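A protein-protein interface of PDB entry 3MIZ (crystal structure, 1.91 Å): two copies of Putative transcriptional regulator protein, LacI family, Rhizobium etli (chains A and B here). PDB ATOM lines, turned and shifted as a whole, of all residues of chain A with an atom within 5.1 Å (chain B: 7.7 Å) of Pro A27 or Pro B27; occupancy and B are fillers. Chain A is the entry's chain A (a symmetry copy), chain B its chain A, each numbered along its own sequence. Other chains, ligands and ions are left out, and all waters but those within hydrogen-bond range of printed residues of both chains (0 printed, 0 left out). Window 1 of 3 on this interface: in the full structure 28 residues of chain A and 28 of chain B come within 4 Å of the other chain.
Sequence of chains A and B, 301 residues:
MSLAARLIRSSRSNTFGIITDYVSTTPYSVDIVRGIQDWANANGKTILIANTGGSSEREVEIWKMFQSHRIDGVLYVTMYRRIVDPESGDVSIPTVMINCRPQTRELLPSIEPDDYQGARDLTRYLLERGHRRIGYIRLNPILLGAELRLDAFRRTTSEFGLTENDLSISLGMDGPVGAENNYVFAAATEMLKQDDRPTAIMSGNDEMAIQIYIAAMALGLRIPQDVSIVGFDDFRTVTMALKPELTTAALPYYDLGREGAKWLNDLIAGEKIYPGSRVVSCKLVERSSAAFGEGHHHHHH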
ATOM      1  N   VAL A  23      23.083  -4.282  11.053  1.00  0.00           N
ATOM      2  CA  VAL A  23      23.796  -5.542  10.882  1.00  0.00           C
ATOM      3  C   VAL A  23      23.349  -6.355   9.659  1.00  0.00           C
ATOM      4  O   VAL A  23      24.156  -7.078   9.067  1.00  0.00           O
ATOM      5  CB  VAL A  23      23.667  -6.428  12.158  1.00  0.00           C
ATOM      6  CG1 VAL A  23      22.276  -7.023  12.250  1.00  0.00           C
ATOM      7  CG2 VAL A  23      24.725  -7.509  12.157  1.00  0.00           C
ATOM      8  N   THR A  25      22.636  -5.226   6.826  1.00  0.00           N
ATOM      9  CA  THR A  25      23.144  -4.588   5.617  1.00  0.00           C
ATOM     10  C   THR A  25      24.604  -4.155   5.774  1.00  0.00           C
ATOM     11  O   THR A  25      25.214  -3.656   4.827  1.00  0.00           O
ATOM     12  CB  THR A  25      22.295  -3.361   5.238  1.00  0.00           C
ATOM     13  OG1 THR A  25      22.847  -2.742   4.070  1.00  0.00           O
ATOM     14  CG2 THR A  25      22.264  -2.358   6.383  1.00  0.00           C
ATOM     15  N   THR A  26      25.153  -4.354   6.971  1.00  0.00           N
ATOM     16  CA  THR A  26      26.545  -4.006   7.276  1.00  0.00           C
ATOM     17  C   THR A  26      27.195  -5.162   8.041  1.00  0.00           C
ATOM     18  O   THR A  26      27.070  -5.254   9.259  1.00  0.00           O
ATOM     19  CB  THR A  26      26.633  -2.722   8.147  1.00  0.00           C
ATOM     20  OG1 THR A  26      26.111  -1.605   7.415  1.00  0.00           O
ATOM     21  CG2 THR A  26      28.076  -2.427   8.529  1.00  0.00           C
ATOM     22  N   PRO A  27      27.888  -6.069   7.331  1.00  0.00           N
ATOM     23  CA  PRO A  27      28.547  -7.215   7.972  1.00  0.00           C
ATOM     24  C   PRO A  27      30.051  -7.030   8.194  1.00  0.00           C
ATOM     25  O   PRO A  27      30.800  -8.010   8.246  1.00  0.00           O
ATOM     26  CB  PRO A  27      28.270  -8.369   7.002  1.00  0.00           C
ATOM     27  CG  PRO A  27      27.371  -7.781   5.918  1.00  0.00           C
ATOM     28  CD  PRO A  27      27.720  -6.331   5.898  1.00  0.00           C
ATOM     29  N   TYR A  28      30.497  -5.786   8.326  1.00  0.00           N
ATOM     30  CA  TYR A  28      31.916  -5.513   8.528  1.00  0.00           C
ATOM     31  C   TYR A  28      32.186  -5.144   9.981  1.00  0.00           C
ATOM     32  O   TYR A  28      33.240  -4.602  10.309  1.00  0.00           O
ATOM     33  CB  TYR A  28      32.369  -4.352   7.640  1.00  0.00           C
ATOM     34  CG  TYR A  28      31.643  -4.258   6.318  1.00  0.00           C
ATOM     35  CD1 TYR A  28      31.562  -5.354   5.461  1.00  0.00           C
ATOM     36  CD2 TYR A  28      31.050  -3.063   5.917  1.00  0.00           C
ATOM     37  CE1 TYR A  28      30.906  -5.261   4.235  1.00  0.00           C
ATOM     38  CE2 TYR A  28      30.392  -2.958   4.695  1.00  0.00           C
ATOM     39  CZ  TYR A  28      30.323  -4.060   3.859  1.00  0.00           C
ATOM     40  OH  TYR A  28      29.677  -3.954   2.650  1.00  0.00           O
ATOM     41  N   SER A  29      31.231  -5.438  10.853  1.00  0.00           N
ATOM     42  CA  SER A  29      31.394  -5.098  12.255  1.00  0.00           C
ATOM     43  C   SER A  29      30.995  -6.247  13.157  1.00  0.00           C
ATOM     44  O   SER A  29      30.914  -6.093  14.378  1.00  0.00           O
ATOM     45  CB  SER A  29      30.562  -3.867  12.566  1.00  0.00           C
ATOM     46  OG  SER A  29      30.800  -2.878  11.586  1.00  0.00           O
ATOM     47  N   VAL A  30      30.758  -7.398  12.539  1.00  0.00           N
ATOM     48  CA  VAL A  30      30.369  -8.598  13.259  1.00  0.00           C
ATOM     49  C   VAL A  30      31.430  -8.981  14.275  1.00  0.00           C
ATOM     50  O   VAL A  30      31.139  -9.691  15.236  1.00  0.00           O
ATOM     51  CB  VAL A  30      30.155  -9.787  12.300  1.00  0.00           C
ATOM     52  CG1 VAL A  30      29.060  -9.456  11.297  1.00  0.00           C
ATOM     53  CG2 VAL A  30      31.455 -10.120  11.585  1.00  0.00           C
ATOM     54  N   PHE A 235      39.901  -5.142   7.458  1.00  0.00           N
ATOM     55  CA  PHE A 235      38.761  -5.976   7.092  1.00  0.00           C
ATOM     56  C   PHE A 235      39.434  -7.185   6.451  1.00  0.00           C
ATOM     57  O   PHE A 235      39.802  -7.139   5.281  1.00  0.00           O
ATOM     58  CB  PHE A 235      37.883  -5.220   6.083  1.00  0.00           C
ATOM     59  CG  PHE A 235      36.692  -5.999   5.581  1.00  0.00           C
ATOM     60  CD1 PHE A 235      36.047  -6.932   6.385  1.00  0.00           C
ATOM     61  CD2 PHE A 235      36.189  -5.756   4.305  1.00  0.00           C
ATOM     62  CE1 PHE A 235      34.916  -7.614   5.927  1.00  0.00           C
ATOM     63  CE2 PHE A 235      35.057  -6.431   3.837  1.00  0.00           C
ATOM     64  CZ  PHE A 235      34.420  -7.360   4.652  1.00  0.00           C
ATOM     65  N   TYR B  22      27.619 -19.728  12.527  1.00  0.00           N
ATOM     66  CA  TYR B  22      28.852 -18.940  12.491  1.00  0.00           C
ATOM     67  C   TYR B  22      28.751 -17.496  12.031  1.00  0.00           C
ATOM     68  O   TYR B  22      29.653 -16.998  11.354  1.00  0.00           O
ATOM     69  CB  TYR B  22      29.871 -19.669  11.618  1.00  0.00           C
ATOM     70  CG  TYR B  22      30.051 -21.116  12.002  1.00  0.00           C
ATOM     71  CD1 TYR B  22      30.735 -21.470  13.166  1.00  0.00           C
ATOM     72  CD2 TYR B  22      29.513 -22.132  11.219  1.00  0.00           C
ATOM     73  CE1 TYR B  22      30.877 -22.803  13.540  1.00  0.00           C
ATOM     74  CE2 TYR B  22      29.648 -23.469  11.583  1.00  0.00           C
ATOM     75  CZ  TYR B  22      30.333 -23.795  12.748  1.00  0.00           C
ATOM     76  OH  TYR B  22      30.454 -25.114  13.119  1.00  0.00           O
ATOM     77  N   VAL B  23      27.684 -16.813  12.421  1.00  0.00           N
ATOM     78  CA  VAL B  23      27.483 -15.428  12.012  1.00  0.00           C
ATOM     79  C   VAL B  23      28.562 -14.462  12.518  1.00  0.00           C
ATOM     80  O   VAL B  23      28.866 -13.468  11.852  1.00  0.00           O
ATOM     81  CB  VAL B  23      26.083 -14.915  12.467  1.00  0.00           C
ATOM     82  CG1 VAL B  23      26.074 -14.661  13.961  1.00  0.00           C
ATOM     83  CG2 VAL B  23      25.705 -13.669  11.697  1.00  0.00           C
ATOM     84  N   SER B  24      29.154 -14.752  13.678  1.00  0.00           N
ATOM     85  CA  SER B  24      30.174 -13.863  14.230  1.00  0.00           C
ATOM     86  C   SER B  24      31.508 -13.983  13.501  1.00  0.00           C
ATOM     87  O   SER B  24      32.399 -13.159  13.691  1.00  0.00           O
ATOM     88  CB  SER B  24      30.383 -14.141  15.721  1.00  0.00           C
ATOM     89  OG  SER B  24      31.018 -15.393  15.930  1.00  0.00           O
ATOM     90  N   THR B  25      31.641 -15.014  12.673  1.00  0.00           N
ATOM     91  CA  THR B  25      32.869 -15.229  11.916  1.00  0.00           C
ATOM     92  C   THR B  25      32.594 -15.373  10.417  1.00  0.00           C
ATOM     93  O   THR B  25      33.525 -15.498   9.618  1.00  0.00           O
ATOM     94  CB  THR B  25      33.615 -16.481  12.412  1.00  0.00           C
ATOM     95  OG1 THR B  25      34.793 -16.680  11.621  1.00  0.00           O
ATOM     96  CG2 THR B  25      32.720 -17.710  12.314  1.00  0.00           C
ATOM     97  N   THR B  26      31.315 -15.353  10.047  1.00  0.00           N
ATOM     98  CA  THR B  26      30.889 -15.465   8.648  1.00  0.00           C
ATOM     99  C   THR B  26      29.813 -14.413   8.363  1.00  0.00           C
ATOM    100  O   THR B  26      28.634 -14.638   8.623  1.00  0.00           O
ATOM    101  CB  THR B  26      30.300 -16.871   8.342  1.00  0.00           C
ATOM    102  OG1 THR B  26      31.318 -17.867   8.514  1.00  0.00           O
ATOM    103  CG2 THR B  26      29.783 -16.940   6.915  1.00  0.00           C
ATOM    104  N   PRO B  27      30.211 -13.240   7.840  1.00  0.00           N
ATOM    105  CA  PRO B  27      29.256 -12.167   7.533  1.00  0.00           C
ATOM    106  C   PRO B  27      28.860 -12.080   6.056  1.00  0.00           C
ATOM    107  O   PRO B  27      28.497 -11.007   5.568  1.00  0.00           O
ATOM    108  CB  PRO B  27      29.995 -10.899   7.981  1.00  0.00           C
ATOM    109  CG  PRO B  27      31.296 -11.391   8.608  1.00  0.00           C
ATOM    110  CD  PRO B  27      31.567 -12.688   7.928  1.00  0.00           C
ATOM    111  N   TYR B  28      28.927 -13.200   5.345  1.00  0.00           N
ATOM    112  CA  TYR B  28      28.581 -13.213   3.927  1.00  0.00           C
ATOM    113  C   TYR B  28      27.213 -13.848   3.717  1.00  0.00           C
ATOM    114  O   TYR B  28      26.855 -14.221   2.602  1.00  0.00           O
ATOM    115  CB  TYR B  28      29.615 -14.011   3.131  1.00  0.00           C
ATOM    116  CG  TYR B  28      31.019 -13.940   3.684  1.00  0.00           C
ATOM    117  CD1 TYR B  28      31.632 -12.715   3.939  1.00  0.00           C
ATOM    118  CD2 TYR B  28      31.742 -15.103   3.939  1.00  0.00           C
ATOM    119  CE1 TYR B  28      32.933 -12.650   4.436  1.00  0.00           C
ATOM    120  CE2 TYR B  28      33.042 -15.052   4.434  1.00  0.00           C
ATOM    121  CZ  TYR B  28      33.632 -13.823   4.680  1.00  0.00           C
ATOM    122  OH  TYR B  28      34.917 -13.773   5.165  1.00  0.00           O
ATOM    123  N   SER B  29      26.448 -13.973   4.793  1.00  0.00           N
ATOM    124  CA  SER B  29      25.138 -14.593   4.688  1.00  0.00           C
ATOM    125  C   SER B  29      24.085 -13.798   5.431  1.00  0.00           C
ATOM    126  O   SER B  29      22.949 -14.248   5.590  1.00  0.00           O
ATOM    127  CB  SER B  29      25.216 -16.008   5.233  1.00  0.00           C
ATOM    128  OG  SER B  29      26.334 -16.667   4.676  1.00  0.00           O
ATOM    129  N   VAL B  30      24.478 -12.608   5.873  1.00  0.00           N
ATOM    130  CA  VAL B  30      23.589 -11.720   6.600  1.00  0.00           C
ATOM    131  C   VAL B  30      22.373 -11.374   5.761  1.00  0.00           C
ATOM    132  O   VAL B  30      21.337 -10.989   6.302  1.00  0.00           O
ATOM    133  CB  VAL B  30      24.301 -10.409   6.996  1.00  0.00           C
ATOM    134  CG1 VAL B  30      25.499 -10.715   7.881  1.00  0.00           C
ATOM    135  CG2 VAL B  30      24.733  -9.655   5.750  1.00  0.00           C
ATOM    136  N   ASP B  31      22.494 -11.506   4.441  1.00  0.00           N
ATOM    137  CA  ASP B  31      21.370 -11.205   3.561  1.00  0.00           C
ATOM    138  C   ASP B  31      20.162 -12.083   3.883  1.00  0.00           C
ATOM    139  O   ASP B  31      19.022 -11.696   3.630  1.00  0.00           O
ATOM    140  CB  ASP B  31      21.770 -11.377   2.095  1.00  0.00           C
ATOM    141  CG  ASP B  31      21.785 -10.062   1.345  1.00  0.00           C
ATOM    142  OD1 ASP B  31      22.317  -9.071   1.893  1.00  0.00           O
ATOM    143  OD2 ASP B  31      21.269 -10.019   0.209  1.00  0.00           O
ATOM    144  N   MET B  79      25.376 -20.417   8.088  1.00  0.00           N
ATOM    145  CA  MET B  79      26.118 -19.445   7.284  1.00  0.00           C
ATOM    146  C   MET B  79      26.453 -20.003   5.902  1.00  0.00           C
ATOM    147  O   MET B  79      26.444 -19.274   4.907  1.00  0.00           O
ATOM    148  CB  MET B  79      27.390 -19.023   8.017  1.00  0.00           C
ATOM    149  CG  MET B  79      27.122 -18.114   9.198  1.00  0.00           C
ATOM    150  SD  MET B  79      26.228 -16.479   8.635  1.00  0.00           S
ATOM    151  CE  MET B  79      24.383 -16.911   9.097  1.00  0.00           C
ATOM    152  N   GLU B 207      34.762 -13.941  -3.439  1.00  0.00           N
ATOM    153  CA  GLU B 207      35.859 -13.517  -2.594  1.00  0.00           C
ATOM    154  C   GLU B 207      37.201 -13.913  -3.221  1.00  0.00           C
ATOM    155  O   GLU B 207      38.111 -13.092  -3.324  1.00  0.00           O
ATOM    156  CB  GLU B 207      35.714 -14.150  -1.202  1.00  0.00           C
ATOM    157  CG  GLU B 207      36.578 -13.497  -0.161  1.00  0.00           C
ATOM    158  CD  GLU B 207      36.326 -14.039   1.228  1.00  0.00           C
ATOM    159  OE1 GLU B 207      35.141 -14.172   1.607  1.00  0.00           O
ATOM    160  OE2 GLU B 207      37.312 -14.318   1.938  1.00  0.00           O
ATOM    161  N   PHE B 235      28.528 -11.651  -3.985  1.00  0.00           N
ATOM    162  CA  PHE B 235      28.874 -11.010  -2.722  1.00  0.00           C
ATOM    163  C   PHE B 235      29.145  -9.571  -3.149  1.00  0.00           C
ATOM    164  O   PHE B 235      30.232  -9.263  -3.626  1.00  0.00           O
ATOM    165  CB  PHE B 235      30.136 -11.673  -2.147  1.00  0.00           C
ATOM    166  CG  PHE B 235      30.634 -11.063  -0.859  1.00  0.00           C
ATOM    167  CD1 PHE B 235      29.756 -10.501   0.061  1.00  0.00           C
ATOM    168  CD2 PHE B 235      31.992 -11.097  -0.551  1.00  0.00           C
ATOM    169  CE1 PHE B 235      30.222  -9.981   1.273  1.00  0.00           C
ATOM    170  CE2 PHE B 235      32.468 -10.583   0.658  1.00  0.00           C
ATOM    171  CZ  PHE B 235      31.580 -10.024   1.572  1.00  0.00           C
ATOM    172  N   THR B 237      29.992  -6.716  -1.847  1.00  0.00           N
ATOM    173  CA  THR B 237      31.220  -6.055  -1.422  1.00  0.00           C
ATOM    174  C   THR B 237      32.331  -6.260  -2.459  1.00  0.00           C
ATOM    175  O   THR B 237      33.121  -5.358  -2.749  1.00  0.00           O
ATOM    176  CB  THR B 237      31.678  -6.618  -0.062  1.00  0.00           C
ATOM    177  OG1 THR B 237      30.711  -6.276   0.940  1.00  0.00           O
ATOM    178  CG2 THR B 237      33.036  -6.066   0.328  1.00  0.00           C
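Of chain B, only Pro B27 (3.0 Å) and Val B30 (3.2 Å) come within 4 Å of Pro A27. Printed residues of chain B within 4 Å of Tyr A28: Thr B237 (3.1 Å). Printed residues of chain B within 4 Å of Val A30: Val B23, Ser B24 and Pro B27. Of the printed residues of chain A, Val B23 touches Val A30 (3.9 Å). Of chain A, only Pro A27 (3.0 Å) and Val A30 (3.2 Å) come within 4 Å of Pro B27. Of the printed residues of chain A, Val B30 touches Val A23 and Pro A27. Of the printed residues of chain A, Thr B237 touches Tyr A28 (3.1 Å). The nearest residue of chain B that does not touch Pro A27 is Tyr B28 (5.1 Å). The nearest printed residue of chain A that does not touch Pro B27 is Tyr A28 (5.1 Å).
Val A23 touches Val B30, and with the chains exchanged Val A30 touches Val B23. Pro B27 touches its own counterpart, Pro A27. Pro A27 touches Val B30, and with the chains exchanged Val A30 touches Pro B27. 8 positions are printed for both chains.
Along chain B the printed residues that touch a printed residue of chain A span positions 23 to 237. Hydrophobic or aromatic side chains of chain A that line the printed part of chain B: Pro A27, Tyr A28 and Val A30.
Val B30 touches Val A23 (CB to O, 3.9 Å). O of Pro A27 touches CB of Pro B27, at 3.0 Å. CG2 of Val B30 touches CG of Pro A27, 3.2 Å away. CB of Val A30 touches O of Val B23, 3.9 Å away. Ser B24 touches Val A30 (O to CG2, 3.8 Å). Val A30 touches Pro B27 (CG2 to CG, 3.2 Å).
OG1 of Thr B237 sits at hydrogen-bond distance from OH of Tyr A28 (3.1 Å).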
